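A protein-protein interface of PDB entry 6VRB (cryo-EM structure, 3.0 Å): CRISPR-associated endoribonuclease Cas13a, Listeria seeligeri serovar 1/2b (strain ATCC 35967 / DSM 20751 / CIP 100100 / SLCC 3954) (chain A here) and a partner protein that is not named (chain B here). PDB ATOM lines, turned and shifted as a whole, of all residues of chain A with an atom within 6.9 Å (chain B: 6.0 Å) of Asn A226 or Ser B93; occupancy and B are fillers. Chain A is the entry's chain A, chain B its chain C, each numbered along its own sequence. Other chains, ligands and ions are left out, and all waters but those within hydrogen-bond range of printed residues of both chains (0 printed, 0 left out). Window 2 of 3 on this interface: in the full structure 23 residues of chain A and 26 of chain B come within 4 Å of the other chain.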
ATOM      1  N   GLU A 222      28.699 -18.452   5.948  1.00  0.00           N
ATOM      2  CA  GLU A 222      29.579 -17.271   6.151  1.00  0.00           C
ATOM      3  C   GLU A 222      28.718 -16.004   6.122  1.00  0.00           C
ATOM      4  O   GLU A 222      27.816 -15.916   5.272  1.00  0.00           O
ATOM      5  CB  GLU A 222      30.629 -17.207   5.041  1.00  0.00           C
ATOM      6  CG  GLU A 222      31.903 -16.489   5.445  1.00  0.00           C
ATOM      7  CD  GLU A 222      32.823 -17.291   6.351  1.00  0.00           C
ATOM      8  OE1 GLU A 222      32.359 -17.741   7.418  1.00  0.00           O
ATOM      9  OE2 GLU A 222      33.999 -17.473   5.983  1.00  0.00           O
ATOM     10  N   ALA A 223      29.032 -15.044   6.997  1.00  0.00           N
ATOM     11  CA  ALA A 223      28.284 -13.770   7.106  1.00  0.00           C
ATOM     12  C   ALA A 223      28.423 -12.971   5.806  1.00  0.00           C
ATOM     13  O   ALA A 223      29.509 -13.028   5.191  1.00  0.00           O
ATOM     14  CB  ALA A 223      28.806 -12.987   8.285  1.00  0.00           C
ATOM     15  N   LYS A 224      27.372 -12.220   5.450  1.00  0.00           N
ATOM     16  CA  LYS A 224      27.319 -11.390   4.213  1.00  0.00           C
ATOM     17  C   LYS A 224      27.444 -12.287   2.970  1.00  0.00           C
ATOM     18  O   LYS A 224      28.133 -11.900   2.010  1.00  0.00           O
ATOM     19  CB  LYS A 224      28.276 -10.193   4.329  1.00  0.00           C
ATOM     20  CG  LYS A 224      28.654  -9.465   3.044  1.00  0.00           C
ATOM     21  CD  LYS A 224      29.960  -9.958   2.459  1.00  0.00           C
ATOM     22  CE  LYS A 224      30.522  -9.049   1.387  1.00  0.00           C
ATOM     23  NZ  LYS A 224      31.842  -9.518   0.906  1.00  0.00           N
ATOM     24  N   LYS A 225      26.826 -13.473   3.020  1.00  0.00           N
ATOM     25  CA  LYS A 225      26.808 -14.418   1.871  1.00  0.00           C
ATOM     26  C   LYS A 225      25.887 -13.843   0.790  1.00  0.00           C
ATOM     27  O   LYS A 225      24.857 -13.247   1.160  1.00  0.00           O
ATOM     28  CB  LYS A 225      26.252 -15.776   2.307  1.00  0.00           C
ATOM     29  CG  LYS A 225      24.732 -15.873   2.302  1.00  0.00           C
ATOM     30  CD  LYS A 225      24.212 -17.280   2.494  1.00  0.00           C
ATOM     31  CE  LYS A 225      24.272 -18.117   1.236  1.00  0.00           C
ATOM     32  NZ  LYS A 225      23.267 -17.675   0.241  1.00  0.00           N
ATOM     33  N   ASN A 226      26.223 -14.054  -0.486  1.00  0.00           N
ATOM     34  CA  ASN A 226      25.404 -13.538  -1.617  1.00  0.00           C
ATOM     35  C   ASN A 226      24.940 -14.718  -2.480  1.00  0.00           C
ATOM     36  O   ASN A 226      25.802 -15.517  -2.877  1.00  0.00           O
ATOM     37  CB  ASN A 226      26.207 -12.532  -2.442  1.00  0.00           C
ATOM     38  CG  ASN A 226      25.359 -11.740  -3.411  1.00  0.00           C
ATOM     39  OD1 ASN A 226      24.141 -11.871  -3.428  1.00  0.00           O
ATOM     40  ND2 ASN A 226      25.999 -10.911  -4.217  1.00  0.00           N
ATOM     41  N   ASP A 227      23.639 -14.808  -2.781  1.00  0.00           N
ATOM     42  CA  ASP A 227      23.133 -15.900  -3.598  1.00  0.00           C
ATOM     43  C   ASP A 227      23.550 -15.789  -5.055  1.00  0.00           C
ATOM     44  O   ASP A 227      23.391 -16.758  -5.799  1.00  0.00           O
ATOM     45  CB  ASP A 227      21.616 -15.961  -3.510  1.00  0.00           C
ATOM     46  CG  ASP A 227      21.134 -16.317  -2.131  1.00  0.00           C
ATOM     47  OD1 ASP A 227      21.862 -17.040  -1.422  1.00  0.00           O
ATOM     48  OD2 ASP A 227      20.030 -15.872  -1.752  1.00  0.00           O
ATOM     49  N   LYS A 228      24.065 -14.639  -5.479  1.00  0.00           N
ATOM     50  CA  LYS A 228      24.638 -14.515  -6.808  1.00  0.00           C
ATOM     51  C   LYS A 228      26.045 -15.100  -6.878  1.00  0.00           C
ATOM     52  O   LYS A 228      26.517 -15.424  -7.969  1.00  0.00           O
ATOM     53  CB  LYS A 228      24.674 -13.048  -7.215  1.00  0.00           C
ATOM     54  CG  LYS A 228      23.349 -12.313  -7.154  1.00  0.00           C
ATOM     55  CD  LYS A 228      22.410 -12.650  -8.282  1.00  0.00           C
ATOM     56  CE  LYS A 228      21.179 -11.756  -8.217  1.00  0.00           C
ATOM     57  NZ  LYS A 228      20.247 -11.980  -9.347  1.00  0.00           N
ATOM     58  N   GLU A 229      26.721 -15.250  -5.736  1.00  0.00           N
ATOM     59  CA  GLU A 229      28.117 -15.665  -5.687  1.00  0.00           C
ATOM     60  C   GLU A 229      28.373 -17.005  -5.028  1.00  0.00           C
ATOM     61  O   GLU A 229      29.482 -17.522  -5.168  1.00  0.00           O
ATOM     62  CB  GLU A 229      28.958 -14.645  -4.914  1.00  0.00           C
ATOM     63  CG  GLU A 229      29.191 -13.365  -5.602  1.00  0.00           C
ATOM     64  CD  GLU A 229      29.921 -12.367  -4.732  1.00  0.00           C
ATOM     65  OE1 GLU A 229      30.131 -12.659  -3.536  1.00  0.00           O
ATOM     66  OE2 GLU A 229      30.279 -11.283  -5.242  1.00  0.00           O
ATOM     67  N   ILE A 230      27.420 -17.547  -4.269  1.00  0.00           N
ATOM     68  CA  ILE A 230      27.739 -18.615  -3.327  1.00  0.00           C
ATOM     69  C   ILE A 230      28.110 -19.918  -4.026  1.00  0.00           C
ATOM     70  O   ILE A 230      28.889 -20.702  -3.479  1.00  0.00           O
ATOM     71  CB  ILE A 230      26.574 -18.787  -2.334  1.00  0.00           C
ATOM     72  CG1 ILE A 230      26.989 -19.648  -1.140  1.00  0.00           C
ATOM     73  CG2 ILE A 230      25.347 -19.351  -3.013  1.00  0.00           C
ATOM     74  CD1 ILE A 230      28.071 -19.038  -0.294  1.00  0.00           C
ATOM     75  N   ASN A 231      27.665 -20.132  -5.257  1.00  0.00           N
ATOM     76  CA  ASN A 231      28.024 -21.350  -5.961  1.00  0.00           C
ATOM     77  C   ASN A 231      29.448 -21.301  -6.482  1.00  0.00           C
ATOM     78  O   ASN A 231      30.073 -22.349  -6.668  1.00  0.00           O
ATOM     79  CB  ASN A 231      27.052 -21.581  -7.105  1.00  0.00           C
ATOM     80  CG  ASN A 231      25.660 -21.864  -6.626  1.00  0.00           C
ATOM     81  OD1 ASN A 231      25.463 -22.564  -5.647  1.00  0.00           O
ATOM     82  ND2 ASN A 231      24.682 -21.322  -7.321  1.00  0.00           N
ATOM     83  N   LYS A 233      32.049 -19.799  -4.929  1.00  0.00           N
ATOM     84  CA  LYS A 233      33.003 -19.952  -3.850  1.00  0.00           C
ATOM     85  C   LYS A 233      32.759 -21.200  -3.024  1.00  0.00           C
ATOM     86  O   LYS A 233      33.633 -21.589  -2.254  1.00  0.00           O
ATOM     87  CB  LYS A 233      33.021 -18.702  -2.974  1.00  0.00           C
ATOM     88  CG  LYS A 233      31.748 -18.373  -2.281  1.00  0.00           C
ATOM     89  CD  LYS A 233      31.884 -17.005  -1.661  1.00  0.00           C
ATOM     90  CE  LYS A 233      32.906 -17.008  -0.536  1.00  0.00           C
ATOM     91  NZ  LYS A 233      33.001 -15.685   0.137  1.00  0.00           N
ATOM     92  N   ALA B  88      24.196  -3.956 -15.463  1.00  0.00           N
ATOM     93  CA  ALA B  88      22.926  -4.182 -14.790  1.00  0.00           C
ATOM     94  C   ALA B  88      22.940  -5.404 -13.886  1.00  0.00           C
ATOM     95  O   ALA B  88      22.041  -5.549 -13.059  1.00  0.00           O
ATOM     96  CB  ALA B  88      21.806  -4.310 -15.814  1.00  0.00           C
ATOM     97  N   SER B  89      23.916  -6.290 -14.027  1.00  0.00           N
ATOM     98  CA  SER B  89      24.095  -7.368 -13.070  1.00  0.00           C
ATOM     99  C   SER B  89      24.640  -6.876 -11.740  1.00  0.00           C
ATOM    100  O   SER B  89      24.335  -7.471 -10.703  1.00  0.00           O
ATOM    101  CB  SER B  89      25.030  -8.429 -13.646  1.00  0.00           C
ATOM    102  OG  SER B  89      26.325  -7.901 -13.854  1.00  0.00           O
ATOM    103  N   VAL B  90      25.431  -5.803 -11.750  1.00  0.00           N
ATOM    104  CA  VAL B  90      25.866  -5.165 -10.513  1.00  0.00           C
ATOM    105  C   VAL B  90      24.682  -4.517  -9.805  1.00  0.00           C
ATOM    106  O   VAL B  90      24.563  -4.587  -8.580  1.00  0.00           O
ATOM    107  CB  VAL B  90      26.982  -4.153 -10.828  1.00  0.00           C
ATOM    108  CG1 VAL B  90      27.393  -3.371  -9.601  1.00  0.00           C
ATOM    109  CG2 VAL B  90      28.173  -4.870 -11.413  1.00  0.00           C
ATOM    110  N   PHE B  91      23.776  -3.906 -10.570  1.00  0.00           N
ATOM    111  CA  PHE B  91      22.581  -3.280 -10.011  1.00  0.00           C
ATOM    112  C   PHE B  91      21.663  -4.305  -9.355  1.00  0.00           C
ATOM    113  O   PHE B  91      21.101  -4.048  -8.288  1.00  0.00           O
ATOM    114  CB  PHE B  91      21.852  -2.536 -11.127  1.00  0.00           C
ATOM    115  CG  PHE B  91      20.618  -1.822 -10.688  1.00  0.00           C
ATOM    116  CD1 PHE B  91      20.696  -0.609 -10.044  1.00  0.00           C
ATOM    117  CD2 PHE B  91      19.372  -2.359 -10.940  1.00  0.00           C
ATOM    118  CE1 PHE B  91      19.558   0.048  -9.655  1.00  0.00           C
ATOM    119  CE2 PHE B  91      18.237  -1.708 -10.544  1.00  0.00           C
ATOM    120  CZ  PHE B  91      18.328  -0.504  -9.906  1.00  0.00           C
ATOM    121  N   GLU B  92      21.507  -5.474  -9.977  1.00  0.00           N
ATOM    122  CA  GLU B  92      20.666  -6.530  -9.428  1.00  0.00           C
ATOM    123  C   GLU B  92      21.287  -7.193  -8.219  1.00  0.00           C
ATOM    124  O   GLU B  92      20.557  -7.623  -7.328  1.00  0.00           O
ATOM    125  CB  GLU B  92      20.412  -7.601 -10.475  1.00  0.00           C
ATOM    126  CG  GLU B  92      19.558  -7.173 -11.618  1.00  0.00           C
ATOM    127  CD  GLU B  92      19.614  -8.154 -12.762  1.00  0.00           C
ATOM    128  OE1 GLU B  92      20.392  -9.125 -12.676  1.00  0.00           O
ATOM    129  OE2 GLU B  92      18.912  -7.941 -13.767  1.00  0.00           O
ATOM    130  N   SER B  93      22.606  -7.299  -8.175  1.00  0.00           N
ATOM    131  CA  SER B  93      23.270  -7.948  -7.059  1.00  0.00           C
ATOM    132  C   SER B  93      23.362  -7.061  -5.833  1.00  0.00           C
ATOM    133  O   SER B  93      23.291  -7.568  -4.710  1.00  0.00           O
ATOM    134  CB  SER B  93      24.667  -8.391  -7.475  1.00  0.00           C
ATOM    135  OG  SER B  93      25.333  -9.010  -6.402  1.00  0.00           O
ATOM    136  N   VAL B  94      23.500  -5.749  -6.018  1.00  0.00           N
ATOM    137  CA  VAL B  94      23.528  -4.834  -4.885  1.00  0.00           C
ATOM    138  C   VAL B  94      22.148  -4.731  -4.249  1.00  0.00           C
ATOM    139  O   VAL B  94      22.011  -4.730  -3.020  1.00  0.00           O
ATOM    140  CB  VAL B  94      24.078  -3.465  -5.326  1.00  0.00           C
ATOM    141  CG1 VAL B  94      23.896  -2.424  -4.260  1.00  0.00           C
ATOM    142  CG2 VAL B  94      25.546  -3.585  -5.635  1.00  0.00           C
ATOM    143  N   LEU B  95      21.099  -4.703  -5.064  1.00  0.00           N
ATOM    144  CA  LEU B  95      19.746  -4.571  -4.551  1.00  0.00           C
ATOM    145  C   LEU B  95      19.011  -5.899  -4.412  1.00  0.00           C
ATOM    146  O   LEU B  95      17.830  -5.883  -4.059  1.00  0.00           O
ATOM    147  CB  LEU B  95      18.937  -3.633  -5.438  1.00  0.00           C
ATOM    148  CG  LEU B  95      19.409  -2.187  -5.406  1.00  0.00           C
ATOM    149  CD1 LEU B  95      18.640  -1.374  -6.405  1.00  0.00           C
ATOM    150  CD2 LEU B  95      19.237  -1.623  -4.017  1.00  0.00           C
ATOM    151  N   GLN B  96      19.673  -7.022  -4.705  1.00  0.00           N
ATOM    152  CA  GLN B  96      19.184  -8.387  -4.455  1.00  0.00           C
ATOM    153  C   GLN B  96      17.846  -8.667  -5.140  1.00  0.00           C
ATOM    154  O   GLN B  96      16.887  -9.128  -4.527  1.00  0.00           O
ATOM    155  CB  GLN B  96      19.117  -8.671  -2.955  1.00  0.00           C
ATOM    156  CG  GLN B  96      20.487  -8.713  -2.345  1.00  0.00           C
ATOM    157  CD  GLN B  96      21.307  -9.857  -2.896  1.00  0.00           C
ATOM    158  OE1 GLN B  96      20.824 -10.981  -3.011  1.00  0.00           O
ATOM    159  NE2 GLN B  96      22.540  -9.568  -3.283  1.00  0.00           N
ATOM    160  N   ILE B  97      17.815  -8.394  -6.438  1.00  0.00           N
ATOM    161  CA  ILE B  97      16.609  -8.522  -7.247  1.00  0.00           C
ATOM    162  C   ILE B  97      16.586  -9.901  -7.885  1.00  0.00           C
ATOM    163  O   ILE B  97      17.554 -10.313  -8.529  1.00  0.00           O
ATOM    164  CB  ILE B  97      16.561  -7.421  -8.316  1.00  0.00           C
ATOM    165  CG1 ILE B  97      16.538  -6.050  -7.646  1.00  0.00           C
ATOM    166  CG2 ILE B  97      15.372  -7.607  -9.227  1.00  0.00           C
ATOM    167  CD1 ILE B  97      16.816  -4.916  -8.575  1.00  0.00           C
ATOM    168  N   TYR B  98      15.483 -10.622  -7.701  1.00  0.00           N
ATOM    169  CA  TYR B  98      15.324 -11.965  -8.237  1.00  0.00           C
ATOM    170  C   TYR B  98      13.966 -12.039  -8.918  1.00  0.00           C
ATOM    171  O   TYR B  98      13.248 -11.044  -9.026  1.00  0.00           O
ATOM    172  CB  TYR B  98      15.435 -13.013  -7.126  1.00  0.00           C
ATOM    173  CG  TYR B  98      16.763 -13.053  -6.420  1.00  0.00           C
ATOM    174  CD1 TYR B  98      17.810 -13.831  -6.887  1.00  0.00           C
ATOM    175  CD2 TYR B  98      16.971 -12.294  -5.283  1.00  0.00           C
ATOM    176  CE1 TYR B  98      19.024 -13.857  -6.225  1.00  0.00           C
ATOM    177  CE2 TYR B  98      18.177 -12.309  -4.627  1.00  0.00           C
ATOM    178  CZ  TYR B  98      19.193 -13.092  -5.096  1.00  0.00           C
ATOM    179  OH  TYR B  98      20.388 -13.089  -4.429  1.00  0.00           O
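OD1 of Asn A226 lies close to N of Lys A228 (3.4 Å). The backbone carbonyl oxygen of Glu B92 sits at hydrogen-bond distance from the backbone NH of Ile B97 (3.0 Å). The side-chain amide nitrogen (NE2) of Gln B96 lies within hydrogen-bond range of the backbone carbonyl oxygen (O) of Ser B93 (2.6 Å). OE1 of Gln B96 sits at hydrogen-bond distance from OH of Tyr B98, 2.6 Å away.
Printed residues of chain A that touch a printed residue of chain B: Asn A226, Asp A227 and Lys A228. Of the 11 printed residues of chain B, 4 touch a printed residue of chain A. Hydrophobic or aromatic side chains of chain B within 4 Å of the printed part of chain A: Tyr B98. Among the printed residues, 6 pairs touch across the chains.
Asp A227 touches Tyr B98. Lys A228 touches Ser B93. Tyr B98 touches Lys A228.
The side-chain hydroxyl (OG) of Ser B93 is in hydrogen-bond range of the side-chain amide nitrogen (ND2) of Asn A226, 3.0 Å away. The side-chain amide nitrogen (NE2) of Gln B96 lies within hydrogen-bond range of the side-chain amide oxygen (OD1) of Asn A226. The side-chain amino group of Lys A228 sits at hydrogen-bond distance from the backbone carbonyl oxygen of Ile B97 (3.3 Å).
Asn A226 touches just these residues of chain B: Ser B93 and Gln B96. Of the printed residues of chain B, Lys A228 touches Ser B93, Ile B97 and Tyr B98. Lys A233 touches none of the printed residues of chain B. Ser B93 touches two residues of chain A. Printed residues of chain A within 4 Å of Gln B96: Asn A226. The nearest residue of chain B that does not touch Asn A226 is Tyr B98 (4.1 Å). The nearest residue of chain A that does not touch Ser B93 is Glu A229 (5.6 Å). The nearest printed residue of chain A that does not touch Ile B97 is Asn A226 (7.8 Å).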
